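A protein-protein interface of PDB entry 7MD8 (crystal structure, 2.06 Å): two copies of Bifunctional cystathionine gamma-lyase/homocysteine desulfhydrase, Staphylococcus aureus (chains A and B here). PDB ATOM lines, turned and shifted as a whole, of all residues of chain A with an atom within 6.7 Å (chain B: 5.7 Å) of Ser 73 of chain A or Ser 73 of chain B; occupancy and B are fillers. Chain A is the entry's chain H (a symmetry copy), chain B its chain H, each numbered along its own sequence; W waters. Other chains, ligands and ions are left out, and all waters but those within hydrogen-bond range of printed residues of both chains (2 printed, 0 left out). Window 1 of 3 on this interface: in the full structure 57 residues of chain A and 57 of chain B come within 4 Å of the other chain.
Water W1 lies within hydrogen-bond range of the backbone carbonyl oxygen (O) of Ile 230 of chain B (2.8 Å) and the backbone carbonyl oxygen (O) of Ser 73 of chain A (3.2 Å).
Water W2 bridges O of Ile 230 of chain A (2.8 Å) and O of Ser 73 of chain B (3.2 Å).
Hydrophobic or aromatic side chains of chain B within 4 Å of the printed part of chain A: Ala 77 and Ile 230.
Printed residues of chain A that touch a printed residue of chain B: Ser 73, Ser 74, Val 76, Ala 77, Thr 227, Gly 228, Gly 229 and Ile 230.
Hydrophobic or aromatic side chains of chain A within 4 Å of the printed part of chain B: Val 76, Ala 77 and Ile 230.
Ser 73 of chain A touches Gly 228 of chain B, and with the chains exchanged Gly 228 of chain A touches Ser 73 of chain B.
Ser 73 of chain A touches Ile 230 of chain B, and with the chains exchanged Ile 230 of chain A touches Ser 73 of chain B.
Ser 74 of chain A touches Gly 228 of chain B, and with the chains exchanged Gly 228 of chain A touches Ser 74 of chain B.
Ala 77 of chain A touches Gly 228 of chain B, and with the chains exchanged Gly 228 of chain A touches Ala 77 of chain B.
13 positions are printed for both chains.
Of the 13 pairs that touch across the chains among the printed residues, 11 have their exchanged pair printed and touching as well.
Ser 73 of chain B touches Ser 73 of chain A.
OG of Ser 73 of chain A touches CA of Gly 229 of chain B (3.4 Å).
O of Ile 230 of chain B touches CB of Ser 73 of chain A, at 3.5 Å.
Gly 228 of chain B touches Val 76 of chain A (CA to CG2, 3.6 Å).
O of Gly 228 of chain B touches CB of Ala 77 of chain A (3.5 Å).
Gly 228 of chain A touches Ala 77 of chain B.
Ser 73 of chain B touches Gly 229 of chain A.
Ser 73 of chain B touches Ile 230 of chain A.
The backbone carbonyl oxygen of Gly 228 of chain A is in hydrogen-bond range of the side-chain hydroxyl of Ser 73 of chain B (3.0 Å).
The backbone carbonyl oxygen of Gly 228 of chain A sits at hydrogen-bond distance from the side-chain hydroxyl of Ser 74 of chain B, 2.7 Å away.
The backbone NH (N) of Ala 77 of chain B lies close to the backbone carbonyl oxygen (O) of Thr 227 of chain A, at 3.4 Å.
O of Gly 228 of chain B is in hydrogen-bond range of OG of Ser 73 of chain A (3.0 Å).
The backbone carbonyl oxygen (O) of Gly 228 of chain B is in hydrogen-bond range of the side-chain hydroxyl (OG) of Ser 74 of chain A (2.7 Å).
N of Ser 73 of chain B lies within hydrogen-bond range of O of Gly 229 of chain B (2.9 Å).
The backbone NH of Ala 77 of chain B sits at hydrogen-bond distance from the side-chain hydroxyl of Ser 74 of chain B, at 3.0 Å.
N of Gly 207 of chain B sits close to O of Ser 74 of chain B, at 3.4 Å.
The backbone NH (N) of Ser 73 of chain A lies within hydrogen-bond range of the backbone carbonyl oxygen (O) of Gly 229 of chain A.
The backbone carbonyl oxygen (O) of Ser 74 of chain A sits close to the backbone NH (N) of Gly 207 of chain A, at 3.4 Å.
OP3 of LLP 196 of chain A is in hydrogen-bond range of the backbone NH (N) of Val 76 of chain A, 2.8 Å away.
Ser 73 of chain A touches four residues of chain B.
Printed residues of chain B within 4 Å of Ser 74 of chain A: Gly 228.
Of the printed residues of chain B, Ala 77 of chain A touches Gly 228 (3.5 Å).
Ser 73 of chain B touches just these residues of chain A: Ser 73, Gly 228, Gly 229 and Ile 230.
The nearest residue of chain A that does not touch Ser 73 of chain B is Leu 231 of chain A (5.7 Å).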
ATOM      1  N   ARG A  47     -11.761 -11.142 -16.027  1.00  0.00           N
ATOM      2  CA  ARG A  47     -11.909 -10.565 -14.691  1.00  0.00           C
ATOM      3  C   ARG A  47     -13.379 -10.327 -14.374  1.00  0.00           C
ATOM      4  O   ARG A  47     -13.853 -10.665 -13.281  1.00  0.00           O
ATOM      5  CB  ARG A  47     -11.111  -9.264 -14.559  1.00  0.00           C
ATOM      6  CG  ARG A  47     -11.551  -8.425 -13.350  1.00  0.00           C
ATOM      7  CD  ARG A  47     -10.474  -7.488 -12.818  1.00  0.00           C
ATOM      8  NE  ARG A  47      -9.851  -6.661 -13.852  1.00  0.00           N
ATOM      9  CZ  ARG A  47     -10.458  -5.664 -14.488  1.00  0.00           C
ATOM     10  NH1 ARG A  47     -11.714  -5.349 -14.200  1.00  0.00           N
ATOM     11  NH2 ARG A  47      -9.810  -4.989 -15.423  1.00  0.00           N
ATOM     12  N   ALA A  71     -16.813 -16.136  -6.692  1.00  0.00           N
ATOM     13  CA  ALA A  71     -15.606 -16.885  -6.357  1.00  0.00           C
ATOM     14  C   ALA A  71     -14.414 -15.941  -6.297  1.00  0.00           C
ATOM     15  O   ALA A  71     -14.148 -15.195  -7.247  1.00  0.00           O
ATOM     16  CB  ALA A  71     -15.341 -18.007  -7.363  1.00  0.00           C
ATOM     17  N   PHE A  72     -13.690 -15.993  -5.188  1.00  0.00           N
ATOM     18  CA  PHE A  72     -12.546 -15.140  -4.940  1.00  0.00           C
ATOM     19  C   PHE A  72     -11.289 -15.987  -4.823  1.00  0.00           C
ATOM     20  O   PHE A  72     -11.349 -17.199  -4.589  1.00  0.00           O
ATOM     21  CB  PHE A  72     -12.767 -14.310  -3.676  1.00  0.00           C
ATOM     22  CG  PHE A  72     -13.896 -13.320  -3.801  1.00  0.00           C
ATOM     23  CD1 PHE A  72     -15.206 -13.696  -3.524  1.00  0.00           C
ATOM     24  CD2 PHE A  72     -13.650 -12.018  -4.223  1.00  0.00           C
ATOM     25  CE1 PHE A  72     -16.246 -12.782  -3.650  1.00  0.00           C
ATOM     26  CE2 PHE A  72     -14.689 -11.093  -4.350  1.00  0.00           C
ATOM     27  CZ  PHE A  72     -15.989 -11.479  -4.059  1.00  0.00           C
ATOM     28  N   SER A  73     -10.142 -15.322  -4.983  1.00  0.00           N
ATOM     29  CA  SER A  73      -8.839 -15.982  -4.960  1.00  0.00           C
ATOM     30  C   SER A  73      -8.475 -16.578  -3.598  1.00  0.00           C
ATOM     31  O   SER A  73      -7.438 -17.243  -3.495  1.00  0.00           O
ATOM     32  CB  SER A  73      -7.759 -14.979  -5.378  1.00  0.00           C
ATOM     33  OG  SER A  73      -8.034 -13.702  -4.821  1.00  0.00           O
ATOM     34  N   SER A  74      -9.276 -16.350  -2.556  1.00  0.00           N
ATOM     35  CA  SER A  74      -9.017 -16.883  -1.221  1.00  0.00           C
ATOM     36  C   SER A  74     -10.211 -16.553  -0.346  1.00  0.00           C
ATOM     37  O   SER A  74     -11.010 -15.671  -0.670  1.00  0.00           O
ATOM     38  CB  SER A  74      -7.736 -16.298  -0.608  1.00  0.00           C
ATOM     39  OG  SER A  74      -7.846 -14.890  -0.454  1.00  0.00           O
ATOM     40  N   GLY A  75     -10.323 -17.272   0.771  1.00  0.00           N
ATOM     41  CA  GLY A  75     -11.309 -16.900   1.777  1.00  0.00           C
ATOM     42  C   GLY A  75     -11.162 -15.465   2.266  1.00  0.00           C
ATOM     43  O   GLY A  75     -12.161 -14.743   2.425  1.00  0.00           O
ATOM     44  N   VAL A  76      -9.925 -15.022   2.534  1.00  0.00           N
ATOM     45  CA  VAL A  76      -9.833 -13.656   3.052  1.00  0.00           C
ATOM     46  C   VAL A  76     -10.116 -12.648   1.955  1.00  0.00           C
ATOM     47  O   VAL A  76     -10.534 -11.529   2.257  1.00  0.00           O
ATOM     48  CB  VAL A  76      -8.493 -13.321   3.758  1.00  0.00           C
ATOM     49  CG1 VAL A  76      -8.274 -14.232   4.971  1.00  0.00           C
ATOM     50  CG2 VAL A  76      -7.323 -13.348   2.830  1.00  0.00           C
ATOM     51  N   ALA A  77      -9.965 -13.020   0.678  1.00  0.00           N
ATOM     52  CA  ALA A  77     -10.394 -12.097  -0.370  1.00  0.00           C
ATOM     53  C   ALA A  77     -11.913 -11.977  -0.395  1.00  0.00           C
ATOM     54  O   ALA A  77     -12.450 -10.877  -0.576  1.00  0.00           O
ATOM     55  CB  ALA A  77      -9.855 -12.535  -1.732  1.00  0.00           C
ATOM     56  N   ALA A  78     -12.624 -13.093  -0.200  1.00  0.00           N
ATOM     57  CA  ALA A  78     -14.076 -13.030  -0.055  1.00  0.00           C
ATOM     58  C   ALA A  78     -14.472 -12.123   1.108  1.00  0.00           C
ATOM     59  O   ALA A  78     -15.374 -11.280   0.984  1.00  0.00           O
ATOM     60  CB  ALA A  78     -14.641 -14.429   0.159  1.00  0.00           C
ATOM     61  N   THR A 195     -10.948 -23.187   0.398  1.00  0.00           N
ATOM     62  CA  THR A 195      -9.666 -23.815   0.681  1.00  0.00           C
ATOM     63  C   THR A 195      -9.799 -25.040   1.582  1.00  0.00           C
ATOM     64  O   THR A 195      -8.965 -25.942   1.540  1.00  0.00           O
ATOM     65  CB  THR A 195      -8.736 -22.790   1.379  1.00  0.00           C
ATOM     66  OG1 THR A 195      -8.732 -21.574   0.623  1.00  0.00           O
ATOM     67  CG2 THR A 195      -7.310 -23.320   1.518  1.00  0.00           C
ATOM     68  N1  LLP A 196     -12.473 -18.349   7.587  1.00  0.00           N
ATOM     69  C2  LLP A 196     -12.345 -19.542   8.103  1.00  0.00           C
ATOM     70  C2' LLP A 196     -13.406 -20.021   9.041  1.00  0.00           C
ATOM     71  C3  LLP A 196     -11.248 -20.357   7.785  1.00  0.00           C
ATOM     72  O3  LLP A 196     -11.160 -21.617   8.370  1.00  0.00           O
ATOM     73  C4  LLP A 196     -10.265 -19.901   6.916  1.00  0.00           C
ATOM     74  C4' LLP A 196      -9.139 -20.789   6.567  1.00  0.00           C
ATOM     75  C5  LLP A 196     -10.421 -18.592   6.379  1.00  0.00           C
ATOM     76  C6  LLP A 196     -11.554 -17.898   6.765  1.00  0.00           C
ATOM     77  C5' LLP A 196      -9.430 -17.935   5.414  1.00  0.00           C
ATOM     78  OP4 LLP A 196      -9.623 -18.439   4.134  1.00  0.00           O
ATOM     79  P   LLP A 196      -8.341 -18.495   3.134  1.00  0.00           P
ATOM     80  OP1 LLP A 196      -7.221 -19.112   3.914  1.00  0.00           O
ATOM     81  OP2 LLP A 196      -8.764 -19.314   1.933  1.00  0.00           O
ATOM     82  OP3 LLP A 196      -7.990 -17.072   2.767  1.00  0.00           O
ATOM     83  N   LLP A 196     -10.836 -25.046   2.421  1.00  0.00           N
ATOM     84  CA  LLP A 196     -11.002 -26.085   3.421  1.00  0.00           C
ATOM     85  CB  LLP A 196     -11.551 -25.489   4.719  1.00  0.00           C
ATOM     86  CG  LLP A 196     -10.904 -24.122   4.981  1.00  0.00           C
ATOM     87  CD  LLP A 196      -9.448 -24.248   5.440  1.00  0.00           C
ATOM     88  CE  LLP A 196      -8.770 -22.860   5.437  1.00  0.00           C
ATOM     89  NZ  LLP A 196      -9.187 -22.086   6.606  1.00  0.00           N
ATOM     90  C   LLP A 196     -11.911 -27.194   2.869  1.00  0.00           C
ATOM     91  O   LLP A 196     -11.531 -27.842   1.871  1.00  0.00           O
ATOM     92  N   VAL A 205      -6.609 -22.715  -3.032  1.00  0.00           N
ATOM     93  CA  VAL A 205      -6.921 -21.598  -2.145  1.00  0.00           C
ATOM     94  C   VAL A 205      -7.991 -20.770  -2.842  1.00  0.00           C
ATOM     95  O   VAL A 205      -7.782 -20.313  -3.972  1.00  0.00           O
ATOM     96  CB  VAL A 205      -5.670 -20.763  -1.827  1.00  0.00           C
ATOM     97  CG1 VAL A 205      -6.043 -19.475  -1.069  1.00  0.00           C
ATOM     98  CG2 VAL A 205      -4.670 -21.598  -1.037  1.00  0.00           C
ATOM     99  N   ALA A 206      -9.139 -20.588  -2.182  1.00  0.00           N
ATOM    100  CA  ALA A 206     -10.306 -19.987  -2.818  1.00  0.00           C
ATOM    101  C   ALA A 206     -11.316 -19.557  -1.762  1.00  0.00           C
ATOM    102  O   ALA A 206     -11.409 -20.162  -0.691  1.00  0.00           O
ATOM    103  CB  ALA A 206     -10.980 -20.965  -3.788  1.00  0.00           C
ATOM    104  N   GLY A 207     -12.105 -18.544  -2.102  1.00  0.00           N
ATOM    105  CA  GLY A 207     -13.244 -18.160  -1.289  1.00  0.00           C
ATOM    106  C   GLY A 207     -14.519 -18.143  -2.111  1.00  0.00           C
ATOM    107  O   GLY A 207     -14.501 -17.904  -3.315  1.00  0.00           O
ATOM    108  N   THR A 227     -11.840  -4.441  -7.635  1.00  0.00           N
ATOM    109  CA  THR A 227     -10.650  -4.763  -6.854  1.00  0.00           C
ATOM    110  C   THR A 227     -10.008  -6.095  -7.247  1.00  0.00           C
ATOM    111  O   THR A 227      -8.865  -6.351  -6.853  1.00  0.00           O
ATOM    112  CB  THR A 227     -10.981  -4.763  -5.354  1.00  0.00           C
ATOM    113  OG1 THR A 227     -12.064  -5.654  -5.103  1.00  0.00           O
ATOM    114  CG2 THR A 227     -11.397  -3.370  -4.905  1.00  0.00           C
ATOM    115  N   GLY A 228     -10.716  -6.947  -7.990  1.00  0.00           N
ATOM    116  CA  GLY A 228     -10.084  -7.982  -8.799  1.00  0.00           C
ATOM    117  C   GLY A 228      -9.531  -9.196  -8.088  1.00  0.00           C
ATOM    118  O   GLY A 228      -8.641  -9.857  -8.632  1.00  0.00           O
ATOM    119  N   GLY A 229     -10.019  -9.516  -6.894  1.00  0.00           N
ATOM    120  CA  GLY A 229      -9.613 -10.730  -6.209  1.00  0.00           C
ATOM    121  C   GLY A 229     -10.353 -11.971  -6.684  1.00  0.00           C
ATOM    122  O   GLY A 229     -10.943 -12.684  -5.868  1.00  0.00           O
ATOM    123  N   ILE A 230     -10.306 -12.256  -8.006  1.00  0.00           N
ATOM    124  CA  ILE A 230     -11.103 -13.315  -8.630  1.00  0.00           C
ATOM    125  C   ILE A 230     -10.371 -14.653  -8.605  1.00  0.00           C
ATOM    126  O   ILE A 230      -9.146 -14.726  -8.782  1.00  0.00           O
ATOM    127  CB  ILE A 230     -11.457 -12.938 -10.081  1.00  0.00           C
ATOM    128  CG1 ILE A 230     -10.157 -12.674 -10.852  1.00  0.00           C
ATOM    129  CG2 ILE A 230     -12.371 -11.731 -10.089  1.00  0.00           C
ATOM    130  CD1 ILE A 230     -10.260 -12.843 -12.295  1.00  0.00           C
ATOM    131  N   LEU A 231     -11.136 -15.726  -8.431  1.00  0.00           N
ATOM    132  CA  LEU A 231     -10.592 -17.068  -8.590  1.00  0.00           C
ATOM    133  C   LEU A 231     -10.331 -17.367 -10.063  1.00  0.00           C
ATOM    134  O   LEU A 231     -11.141 -17.033 -10.927  1.00  0.00           O
ATOM    135  CB  LEU A 231     -11.571 -18.094  -8.023  1.00  0.00           C
ATOM    136  CG  LEU A 231     -11.004 -19.496  -7.837  1.00  0.00           C
ATOM    137  CD1 LEU A 231      -9.875 -19.433  -6.805  1.00  0.00           C
ATOM    138  CD2 LEU A 231     -12.106 -20.452  -7.405  1.00  0.00           C
ATOM    139  N   GLY A 232      -9.199 -18.018 -10.356  1.00  0.00           N
ATOM    140  CA  GLY A 232      -8.878 -18.391 -11.724  1.00  0.00           C
ATOM    141  C   GLY A 232      -9.630 -19.630 -12.180  1.00  0.00           C
ATOM    142  O   GLY A 232     -10.224 -20.379 -11.383  1.00  0.00           O
ATOM    143  N   ALA B  71       2.669 -11.349  -6.956  1.00  0.00           N
ATOM    144  CA  ALA B  71       1.729 -11.726  -8.006  1.00  0.00           C
ATOM    145  C   ALA B  71       0.310 -11.711  -7.457  1.00  0.00           C
ATOM    146  O   ALA B  71       0.018 -12.349  -6.439  1.00  0.00           O
ATOM    147  CB  ALA B  71       2.057 -13.102  -8.590  1.00  0.00           C
ATOM    148  N   PHE B  72      -0.571 -11.001  -8.147  1.00  0.00           N
ATOM    149  CA  PHE B  72      -1.954 -10.840  -7.752  1.00  0.00           C
ATOM    150  C   PHE B  72      -2.864 -11.460  -8.801  1.00  0.00           C
ATOM    151  O   PHE B  72      -2.463 -11.685  -9.948  1.00  0.00           O
ATOM    152  CB  PHE B  72      -2.282  -9.362  -7.548  1.00  0.00           C
ATOM    153  CG  PHE B  72      -1.535  -8.738  -6.397  1.00  0.00           C
ATOM    154  CD1 PHE B  72      -0.261  -8.211  -6.578  1.00  0.00           C
ATOM    155  CD2 PHE B  72      -2.098  -8.705  -5.126  1.00  0.00           C
ATOM    156  CE1 PHE B  72       0.428  -7.644  -5.511  1.00  0.00           C
ATOM    157  CE2 PHE B  72      -1.413  -8.135  -4.050  1.00  0.00           C
ATOM    158  CZ  PHE B  72      -0.147  -7.603  -4.248  1.00  0.00           C
ATOM    159  N   SER B  73      -4.105 -11.726  -8.387  1.00  0.00           N
ATOM    160  CA  SER B  73      -5.099 -12.374  -9.241  1.00  0.00           C
ATOM    161  C   SER B  73      -5.523 -11.526 -10.444  1.00  0.00           C
ATOM    162  O   SER B  73      -6.285 -12.019 -11.283  1.00  0.00           O
ATOM    163  CB  SER B  73      -6.335 -12.718  -8.405  1.00  0.00           C
ATOM    164  OG  SER B  73      -6.611 -11.671  -7.485  1.00  0.00           O
ATOM    165  N   SER B  74      -5.072 -10.275 -10.545  1.00  0.00           N
ATOM    166  CA  SER B  74      -5.414  -9.394 -11.659  1.00  0.00           C
ATOM    167  C   SER B  74      -4.599  -8.121 -11.516  1.00  0.00           C
ATOM    168  O   SER B  74      -4.082  -7.818 -10.439  1.00  0.00           O
ATOM    169  CB  SER B  74      -6.912  -9.060 -11.688  1.00  0.00           C
ATOM    170  OG  SER B  74      -7.300  -8.369 -10.509  1.00  0.00           O
ATOM    171  N   GLY B  75      -4.493  -7.379 -12.618  1.00  0.00           N
ATOM    172  CA  GLY B  75      -3.912  -6.045 -12.540  1.00  0.00           C
ATOM    173  C   GLY B  75      -4.614  -5.137 -11.539  1.00  0.00           C
ATOM    174  O   GLY B  75      -3.959  -4.407 -10.775  1.00  0.00           O
ATOM    175  N   ALA B  77      -6.186  -6.005  -8.948  1.00  0.00           N
ATOM    176  CA  ALA B  77      -5.872  -6.436  -7.588  1.00  0.00           C
ATOM    177  C   ALA B  77      -4.505  -5.921  -7.158  1.00  0.00           C
ATOM    178  O   ALA B  77      -4.328  -5.497  -6.009  1.00  0.00           O
ATOM    179  CB  ALA B  77      -5.947  -7.959  -7.473  1.00  0.00           C
ATOM    180  N   VAL B 205      -5.368 -13.907 -16.425  1.00  0.00           N
ATOM    181  CA  VAL B 205      -5.626 -12.621 -15.784  1.00  0.00           C
ATOM    182  C   VAL B 205      -4.763 -12.574 -14.530  1.00  0.00           C
ATOM    183  O   VAL B 205      -4.872 -13.458 -13.672  1.00  0.00           O
ATOM    184  CB  VAL B 205      -7.117 -12.442 -15.457  1.00  0.00           C
ATOM    185  CG1 VAL B 205      -7.348 -11.185 -14.597  1.00  0.00           C
ATOM    186  CG2 VAL B 205      -7.932 -12.388 -16.743  1.00  0.00           C
ATOM    187  N   ALA B 206      -3.899 -11.559 -14.430  1.00  0.00           N
ATOM    188  CA  ALA B 206      -2.886 -11.512 -13.382  1.00  0.00           C
ATOM    189  C   ALA B 206      -2.312 -10.106 -13.270  1.00  0.00           C
ATOM    190  O   ALA B 206      -2.250  -9.367 -14.257  1.00  0.00           O
ATOM    191  CB  ALA B 206      -1.746 -12.500 -13.661  1.00  0.00           C
ATOM    192  N   GLY B 207      -1.842  -9.772 -12.074  1.00  0.00           N
ATOM    193  CA  GLY B 207      -1.083  -8.552 -11.868  1.00  0.00           C
ATOM    194  C   GLY B 207       0.258  -8.847 -11.223  1.00  0.00           C
ATOM    195  O   GLY B 207       0.412  -9.813 -10.480  1.00  0.00           O
ATOM    196  N   GLY B 228      -5.675 -11.063   0.365  1.00  0.00           N
ATOM    197  CA  GLY B 228      -5.755 -12.355  -0.305  1.00  0.00           C
ATOM    198  C   GLY B 228      -6.018 -12.364  -1.794  1.00  0.00           C
ATOM    199  O   GLY B 228      -6.513 -13.371  -2.310  1.00  0.00           O
ATOM    200  N   GLY B 229      -5.710 -11.284  -2.505  1.00  0.00           N
ATOM    201  CA  GLY B 229      -5.832 -11.268  -3.952  1.00  0.00           C
ATOM    202  C   GLY B 229      -4.648 -11.900  -4.667  1.00  0.00           C
ATOM    203  O   GLY B 229      -4.040 -11.262  -5.530  1.00  0.00           O
ATOM    204  N   ILE B 230      -4.326 -13.172  -4.335  1.00  0.00           N
ATOM    205  CA  ILE B 230      -3.118 -13.847  -4.813  1.00  0.00           C
ATOM    206  C   ILE B 230      -3.364 -14.558  -6.140  1.00  0.00           C
ATOM    207  O   ILE B 230      -4.434 -15.137  -6.378  1.00  0.00           O
ATOM    208  CB  ILE B 230      -2.614 -14.856  -3.764  1.00  0.00           C
ATOM    209  CG1 ILE B 230      -3.740 -15.852  -3.458  1.00  0.00           C
ATOM    210  CG2 ILE B 230      -2.160 -14.120  -2.521  1.00  0.00           C
ATOM    211  CD1 ILE B 230      -3.293 -17.138  -2.940  1.00  0.00           C
ATOM    212  N   LEU B 231      -2.345 -14.555  -6.994  1.00  0.00           N
ATOM    213  CA  LEU B 231      -2.378 -15.365  -8.204  1.00  0.00           C
ATOM    214  C   LEU B 231      -2.218 -16.844  -7.861  1.00  0.00           C
ATOM    215  O   LEU B 231      -1.401 -17.209  -7.016  1.00  0.00           O
ATOM    216  CB  LEU B 231      -1.259 -14.933  -9.149  1.00  0.00           C
ATOM    217  CG  LEU B 231      -1.365 -15.473 -10.569  1.00  0.00           C
ATOM    218  CD1 LEU B 231      -2.641 -14.918 -11.209  1.00  0.00           C
ATOM    219  CD2 LEU B 231      -0.127 -15.093 -11.366  1.00  0.00           C
HETATM  220  O   HOH W   1      -5.973 -17.514  -6.275  1.00  0.00           O
HETATM  221  O   HOH W   2      -6.975 -15.016 -10.579  1.00  0.00           O
